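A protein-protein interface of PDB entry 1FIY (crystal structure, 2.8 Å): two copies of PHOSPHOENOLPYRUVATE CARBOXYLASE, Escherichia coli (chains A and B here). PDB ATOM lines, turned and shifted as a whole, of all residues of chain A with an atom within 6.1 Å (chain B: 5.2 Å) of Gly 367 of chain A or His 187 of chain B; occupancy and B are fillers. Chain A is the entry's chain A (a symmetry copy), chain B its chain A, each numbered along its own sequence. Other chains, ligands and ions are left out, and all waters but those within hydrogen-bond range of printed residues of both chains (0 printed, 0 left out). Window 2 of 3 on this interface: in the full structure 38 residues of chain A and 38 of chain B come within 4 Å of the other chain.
O of Ala 183 of chain B is in hydrogen-bond range of ND1 of His 187 of chain B (3.5 Å).
The side-chain hydroxyl (OG1) of Thr 188 of chain B is in hydrogen-bond range of the backbone carbonyl oxygen (O) of Gln 184 of chain B, at 2.5 Å.
O of Leu 363 of chain A lies within hydrogen-bond range of N of Met 368 of chain A, at 2.7 Å.
Ser 291 of chain A touches Thr 188 of chain B.
CE of Met 292 of chain A touches OG1 of Thr 188 of chain B, at 3.98 Å.
Gly 367 of chain A touches His 187 of chain B (O to NE2, 3.96 Å).
Met 368 of chain A touches His 187 of chain B.
Ile 370 of chain A touches Asp 25 of chain B (CD1 to OD2, 3.9 Å).
Ile 371 of chain A touches Ala 183 of chain B (CD1 to C, 3.9 Å).
Ile 371 of chain A touches Gln 184 of chain B (CD1 to N, 3.6 Å).
Hydrophobic or aromatic side chains of chain B that line the printed part of chain A: His 187.
Along chain B the printed residues that touch a printed residue of chain A span positions 25 to 188.
Among the printed residues, no Asp or Glu carboxylate lies within 4 Å of a Lys or Arg side-chain nitrogen of the other chain.
Of the printed residues of chain B, Ser 291 of chain A touches Thr 188.
Gly 367 of chain A touches just one residue of chain B: His 187.
Printed residues of chain A within 4 Å of Asp 25 of chain B: Ile 370 (3.9 Å).
Printed residues of chain A within 4 Å of Ala 183 of chain B: Ile 371 (3.9 Å).
Of the printed residues of chain A, Gln 184 of chain B touches Ile 371.
His 187 of chain B touches just these residues of chain A: Gly 367 (3.96 Å) and Met 368 (3.6 Å).
Printed residues of chain A within 4 Å of Thr 188 of chain B: Ser 291 (3.1 Å) and Met 292 (3.98 Å).
The nearest residue of chain A that does not touch His 187 of chain B is Ile 371 of chain A (4.2 Å).
The nearest printed residue of chain A that does not touch Asp 25 of chain B is Gly 367 of chain A (5.1 Å).
No position is printed for both chains.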
ATOM      1  N   SER A 291     -24.434  -7.631  -6.413  1.00  0.00           N
ATOM      2  CA  SER A 291     -25.860  -7.853  -6.437  1.00  0.00           C
ATOM      3  C   SER A 291     -26.452  -7.587  -7.818  1.00  0.00           C
ATOM      4  O   SER A 291     -27.665  -7.585  -7.973  1.00  0.00           O
ATOM      5  CB  SER A 291     -26.563  -6.934  -5.421  1.00  0.00           C
ATOM      6  OG  SER A 291     -25.786  -6.793  -4.251  1.00  0.00           O
ATOM      7  N   MET A 292     -25.628  -7.348  -8.816  1.00  0.00           N
ATOM      8  CA  MET A 292     -26.046  -7.103 -10.187  1.00  0.00           C
ATOM      9  C   MET A 292     -26.815  -8.324 -10.693  1.00  0.00           C
ATOM     10  O   MET A 292     -26.537  -9.443 -10.248  1.00  0.00           O
ATOM     11  CB  MET A 292     -24.820  -6.930 -11.086  1.00  0.00           C
ATOM     12  CG  MET A 292     -23.852  -5.856 -10.704  1.00  0.00           C
ATOM     13  SD  MET A 292     -23.018  -6.120  -9.135  1.00  0.00           S
ATOM     14  CE  MET A 292     -22.997  -4.428  -8.507  1.00  0.00           C
ATOM     15  N   GLU A 294     -27.839  -8.333 -14.219  1.00  0.00           N
ATOM     16  CA  GLU A 294     -27.650  -8.342 -15.671  1.00  0.00           C
ATOM     17  C   GLU A 294     -26.291  -8.967 -15.987  1.00  0.00           C
ATOM     18  O   GLU A 294     -25.274  -8.497 -15.500  1.00  0.00           O
ATOM     19  CB  GLU A 294     -27.741  -6.956 -16.267  1.00  0.00           C
ATOM     20  CG  GLU A 294     -28.847  -6.096 -15.683  1.00  0.00           C
ATOM     21  CD  GLU A 294     -28.761  -4.676 -16.205  1.00  0.00           C
ATOM     22  OE1 GLU A 294     -27.702  -4.301 -16.764  1.00  0.00           O
ATOM     23  OE2 GLU A 294     -29.767  -3.949 -16.051  1.00  0.00           O
ATOM     24  N   SER A 362     -18.482  -9.863 -17.879  1.00  0.00           N
ATOM     25  CA  SER A 362     -19.901  -9.517 -18.010  1.00  0.00           C
ATOM     26  C   SER A 362     -20.153  -8.128 -17.436  1.00  0.00           C
ATOM     27  O   SER A 362     -20.845  -7.338 -18.092  1.00  0.00           O
ATOM     28  CB  SER A 362     -20.842 -10.554 -17.435  1.00  0.00           C
ATOM     29  OG  SER A 362     -20.264 -11.262 -16.364  1.00  0.00           O
ATOM     30  N   LEU A 363     -19.573  -7.810 -16.278  1.00  0.00           N
ATOM     31  CA  LEU A 363     -19.755  -6.464 -15.729  1.00  0.00           C
ATOM     32  C   LEU A 363     -19.370  -5.426 -16.774  1.00  0.00           C
ATOM     33  O   LEU A 363     -20.142  -4.489 -17.026  1.00  0.00           O
ATOM     34  CB  LEU A 363     -19.014  -6.278 -14.417  1.00  0.00           C
ATOM     35  CG  LEU A 363     -19.694  -6.901 -13.192  1.00  0.00           C
ATOM     36  CD1 LEU A 363     -18.827  -6.879 -11.958  1.00  0.00           C
ATOM     37  CD2 LEU A 363     -21.053  -6.276 -12.920  1.00  0.00           C
ATOM     38  N   GLN A 364     -18.224  -5.580 -17.434  1.00  0.00           N
ATOM     39  CA  GLN A 364     -17.814  -4.651 -18.482  1.00  0.00           C
ATOM     40  C   GLN A 364     -18.825  -4.653 -19.618  1.00  0.00           C
ATOM     41  O   GLN A 364     -19.391  -3.624 -19.987  1.00  0.00           O
ATOM     42  CB  GLN A 364     -16.420  -4.997 -18.991  1.00  0.00           C
ATOM     43  CG  GLN A 364     -15.331  -4.729 -17.948  1.00  0.00           C
ATOM     44  CD  GLN A 364     -14.672  -3.392 -18.191  1.00  0.00           C
ATOM     45  OE1 GLN A 364     -14.526  -2.990 -19.351  1.00  0.00           O
ATOM     46  NE2 GLN A 364     -14.270  -2.674 -17.152  1.00  0.00           N
ATOM     47  N   ALA A 365     -19.095  -5.827 -20.162  1.00  0.00           N
ATOM     48  CA  ALA A 365     -20.027  -6.051 -21.243  1.00  0.00           C
ATOM     49  C   ALA A 365     -21.392  -5.410 -21.011  1.00  0.00           C
ATOM     50  O   ALA A 365     -21.966  -4.784 -21.896  1.00  0.00           O
ATOM     51  CB  ALA A 365     -20.274  -7.563 -21.381  1.00  0.00           C
ATOM     52  N   CYS A 366     -21.919  -5.608 -19.806  1.00  0.00           N
ATOM     53  CA  CYS A 366     -23.215  -5.119 -19.410  1.00  0.00           C
ATOM     54  C   CYS A 366     -23.266  -3.701 -18.894  1.00  0.00           C
ATOM     55  O   CYS A 366     -24.277  -3.330 -18.270  1.00  0.00           O
ATOM     56  CB  CYS A 366     -23.817  -6.093 -18.377  1.00  0.00           C
ATOM     57  SG  CYS A 366     -24.525  -7.597 -19.108  1.00  0.00           S
ATOM     58  N   GLY A 367     -22.282  -2.848 -19.103  1.00  0.00           N
ATOM     59  CA  GLY A 367     -22.350  -1.482 -18.631  1.00  0.00           C
ATOM     60  C   GLY A 367     -21.993  -1.233 -17.185  1.00  0.00           C
ATOM     61  O   GLY A 367     -22.257  -0.127 -16.669  1.00  0.00           O
ATOM     62  N   MET A 368     -21.373  -2.188 -16.487  1.00  0.00           N
ATOM     63  CA  MET A 368     -20.999  -1.977 -15.100  1.00  0.00           C
ATOM     64  C   MET A 368     -19.496  -1.879 -14.902  1.00  0.00           C
ATOM     65  O   MET A 368     -18.887  -2.340 -13.941  1.00  0.00           O
ATOM     66  CB  MET A 368     -21.627  -3.011 -14.196  1.00  0.00           C
ATOM     67  CG  MET A 368     -23.061  -2.664 -13.818  1.00  0.00           C
ATOM     68  SD  MET A 368     -24.116  -4.090 -13.745  1.00  0.00           S
ATOM     69  CE  MET A 368     -24.179  -4.624 -15.446  1.00  0.00           C
ATOM     70  N   GLY A 369     -18.880  -1.159 -15.841  1.00  0.00           N
ATOM     71  CA  GLY A 369     -17.470  -0.909 -15.881  1.00  0.00           C
ATOM     72  C   GLY A 369     -16.863  -0.441 -14.580  1.00  0.00           C
ATOM     73  O   GLY A 369     -15.856  -0.999 -14.136  1.00  0.00           O
ATOM     74  N   ILE A 370     -17.452   0.584 -13.967  1.00  0.00           N
ATOM     75  CA  ILE A 370     -16.942   1.149 -12.725  1.00  0.00           C
ATOM     76  C   ILE A 370     -16.960   0.160 -11.576  1.00  0.00           C
ATOM     77  O   ILE A 370     -16.132   0.314 -10.678  1.00  0.00           O
ATOM     78  CB  ILE A 370     -17.662   2.445 -12.283  1.00  0.00           C
ATOM     79  CG1 ILE A 370     -18.567   2.945 -13.388  1.00  0.00           C
ATOM     80  CG2 ILE A 370     -16.646   3.477 -11.828  1.00  0.00           C
ATOM     81  CD1 ILE A 370     -18.502   4.399 -13.789  1.00  0.00           C
ATOM     82  N   ILE A 371     -17.862  -0.811 -11.576  1.00  0.00           N
ATOM     83  CA  ILE A 371     -17.913  -1.813 -10.501  1.00  0.00           C
ATOM     84  C   ILE A 371     -16.833  -2.858 -10.770  1.00  0.00           C
ATOM     85  O   ILE A 371     -16.130  -3.293  -9.865  1.00  0.00           O
ATOM     86  CB  ILE A 371     -19.290  -2.490 -10.429  1.00  0.00           C
ATOM     87  CG1 ILE A 371     -20.383  -1.424 -10.216  1.00  0.00           C
ATOM     88  CG2 ILE A 371     -19.319  -3.592  -9.385  1.00  0.00           C
ATOM     89  CD1 ILE A 371     -20.301  -0.692  -8.899  1.00  0.00           C
ATOM     90  N   THR B  22     -22.574   8.917 -13.465  1.00  0.00           N
ATOM     91  CA  THR B  22     -22.899   7.519 -13.284  1.00  0.00           C
ATOM     92  C   THR B  22     -24.167   7.101 -14.012  1.00  0.00           C
ATOM     93  O   THR B  22     -24.189   6.007 -14.572  1.00  0.00           O
ATOM     94  CB  THR B  22     -23.068   7.155 -11.794  1.00  0.00           C
ATOM     95  OG1 THR B  22     -21.819   7.236 -11.106  1.00  0.00           O
ATOM     96  CG2 THR B  22     -23.636   5.751 -11.672  1.00  0.00           C
ATOM     97  N   ASP B  25     -23.203   7.095 -17.779  1.00  0.00           N
ATOM     98  CA  ASP B  25     -22.524   5.842 -18.085  1.00  0.00           C
ATOM     99  C   ASP B  25     -23.534   4.685 -18.054  1.00  0.00           C
ATOM    100  O   ASP B  25     -23.872   4.045 -19.043  1.00  0.00           O
ATOM    101  CB  ASP B  25     -21.457   5.552 -17.026  1.00  0.00           C
ATOM    102  CG  ASP B  25     -20.034   5.752 -17.478  1.00  0.00           C
ATOM    103  OD1 ASP B  25     -19.613   5.031 -18.411  1.00  0.00           O
ATOM    104  OD2 ASP B  25     -19.305   6.610 -16.916  1.00  0.00           O
ATOM    105  N   ALA B  26     -24.043   4.410 -16.862  1.00  0.00           N
ATOM    106  CA  ALA B  26     -24.988   3.368 -16.582  1.00  0.00           C
ATOM    107  C   ALA B  26     -25.862   2.934 -17.746  1.00  0.00           C
ATOM    108  O   ALA B  26     -25.580   1.908 -18.376  1.00  0.00           O
ATOM    109  CB  ALA B  26     -25.893   3.741 -15.403  1.00  0.00           C
ATOM    110  N   ARG B  73     -35.878   5.800  -8.929  1.00  0.00           N
ATOM    111  CA  ARG B  73     -34.592   5.611  -8.248  1.00  0.00           C
ATOM    112  C   ARG B  73     -33.735   6.869  -8.419  1.00  0.00           C
ATOM    113  O   ARG B  73     -33.135   7.382  -7.465  1.00  0.00           O
ATOM    114  CB  ARG B  73     -33.860   4.367  -8.725  1.00  0.00           C
ATOM    115  CG  ARG B  73     -34.589   3.057  -8.601  1.00  0.00           C
ATOM    116  CD  ARG B  73     -33.760   1.795  -8.670  1.00  0.00           C
ATOM    117  NE  ARG B  73     -32.624   1.770  -7.755  1.00  0.00           N
ATOM    118  CZ  ARG B  73     -31.348   1.776  -8.154  1.00  0.00           C
ATOM    119  NH1 ARG B  73     -31.041   1.793  -9.458  1.00  0.00           N
ATOM    120  NH2 ARG B  73     -30.364   1.762  -7.262  1.00  0.00           N
ATOM    121  N   ALA B 183     -21.459   4.660  -7.910  1.00  0.00           N
ATOM    122  CA  ALA B 183     -21.861   3.645  -8.901  1.00  0.00           C
ATOM    123  C   ALA B 183     -22.459   2.448  -8.169  1.00  0.00           C
ATOM    124  O   ALA B 183     -23.513   1.958  -8.567  1.00  0.00           O
ATOM    125  CB  ALA B 183     -20.694   3.225  -9.759  1.00  0.00           C
ATOM    126  N   GLN B 184     -21.801   2.002  -7.093  1.00  0.00           N
ATOM    127  CA  GLN B 184     -22.317   0.901  -6.293  1.00  0.00           C
ATOM    128  C   GLN B 184     -23.828   1.031  -6.084  1.00  0.00           C
ATOM    129  O   GLN B 184     -24.608   0.177  -6.527  1.00  0.00           O
ATOM    130  CB  GLN B 184     -21.600   0.817  -4.946  1.00  0.00           C
ATOM    131  CG  GLN B 184     -20.579  -0.293  -4.790  1.00  0.00           C
ATOM    132  CD  GLN B 184     -19.317   0.100  -4.045  1.00  0.00           C
ATOM    133  OE1 GLN B 184     -19.177   0.003  -2.819  1.00  0.00           O
ATOM    134  NE2 GLN B 184     -18.321   0.571  -4.785  1.00  0.00           N
ATOM    135  N   SER B 185     -24.275   2.098  -5.431  1.00  0.00           N
ATOM    136  CA  SER B 185     -25.671   2.327  -5.144  1.00  0.00           C
ATOM    137  C   SER B 185     -26.582   2.463  -6.337  1.00  0.00           C
ATOM    138  O   SER B 185     -27.779   2.168  -6.219  1.00  0.00           O
ATOM    139  CB  SER B 185     -25.828   3.575  -4.256  1.00  0.00           C
ATOM    140  OG  SER B 185     -25.253   3.263  -2.988  1.00  0.00           O
ATOM    141  N   TRP B 186     -26.080   2.916  -7.477  1.00  0.00           N
ATOM    142  CA  TRP B 186     -26.951   3.055  -8.636  1.00  0.00           C
ATOM    143  C   TRP B 186     -27.279   1.680  -9.205  1.00  0.00           C
ATOM    144  O   TRP B 186     -28.386   1.389  -9.641  1.00  0.00           O
ATOM    145  CB  TRP B 186     -26.298   3.957  -9.699  1.00  0.00           C
ATOM    146  CG  TRP B 186     -27.201   4.032 -10.894  1.00  0.00           C
ATOM    147  CD1 TRP B 186     -26.932   3.577 -12.142  1.00  0.00           C
ATOM    148  CD2 TRP B 186     -28.532   4.563 -10.927  1.00  0.00           C
ATOM    149  NE1 TRP B 186     -28.016   3.800 -12.968  1.00  0.00           N
ATOM    150  CE2 TRP B 186     -29.012   4.404 -12.244  1.00  0.00           C
ATOM    151  CE3 TRP B 186     -29.364   5.173  -9.984  1.00  0.00           C
ATOM    152  CZ2 TRP B 186     -30.279   4.821 -12.641  1.00  0.00           C
ATOM    153  CZ3 TRP B 186     -30.627   5.581 -10.378  1.00  0.00           C
ATOM    154  CH2 TRP B 186     -31.069   5.400 -11.683  1.00  0.00           C
ATOM    155  N   HIS B 187     -26.269   0.817  -9.199  1.00  0.00           N
ATOM    156  CA  HIS B 187     -26.333  -0.525  -9.733  1.00  0.00           C
ATOM    157  C   HIS B 187     -26.620  -1.571  -8.675  1.00  0.00           C
ATOM    158  O   HIS B 187     -27.276  -2.562  -9.012  1.00  0.00           O
ATOM    159  CB  HIS B 187     -25.025  -0.905 -10.433  1.00  0.00           C
ATOM    160  CG  HIS B 187     -24.730  -0.145 -11.674  1.00  0.00           C
ATOM    161  ND1 HIS B 187     -23.631   0.662 -11.780  1.00  0.00           N
ATOM    162  CD2 HIS B 187     -25.383  -0.070 -12.855  1.00  0.00           C
ATOM    163  CE1 HIS B 187     -23.601   1.214 -12.982  1.00  0.00           C
ATOM    164  NE2 HIS B 187     -24.654   0.780 -13.648  1.00  0.00           N
ATOM    165  N   THR B 188     -26.173  -1.393  -7.439  1.00  0.00           N
ATOM    166  CA  THR B 188     -26.495  -2.389  -6.419  1.00  0.00           C
ATOM    167  C   THR B 188     -27.937  -2.187  -5.953  1.00  0.00           C
ATOM    168  O   THR B 188     -28.163  -1.730  -4.828  1.00  0.00           O
ATOM    169  CB  THR B 188     -25.587  -2.357  -5.188  1.00  0.00           C
ATOM    170  OG1 THR B 188     -24.230  -2.068  -5.543  1.00  0.00           O
ATOM    171  CG2 THR B 188     -25.629  -3.734  -4.511  1.00  0.00           C
ATOM    172  N   ASP B 189     -28.907  -2.510  -6.804  1.00  0.00           N
ATOM    173  CA  ASP B 189     -30.296  -2.335  -6.415  1.00  0.00           C
ATOM    174  C   ASP B 189     -30.847  -3.635  -5.818  1.00  0.00           C
ATOM    175  O   ASP B 189     -30.709  -4.737  -6.339  1.00  0.00           O
ATOM    176  CB  ASP B 189     -31.192  -1.823  -7.516  1.00  0.00           C
ATOM    177  CG  ASP B 189     -31.725  -2.845  -8.495  1.00  0.00           C
ATOM    178  OD1 ASP B 189     -30.916  -3.643  -9.028  1.00  0.00           O
ATOM    179  OD2 ASP B 189     -32.959  -2.858  -8.749  1.00  0.00           O
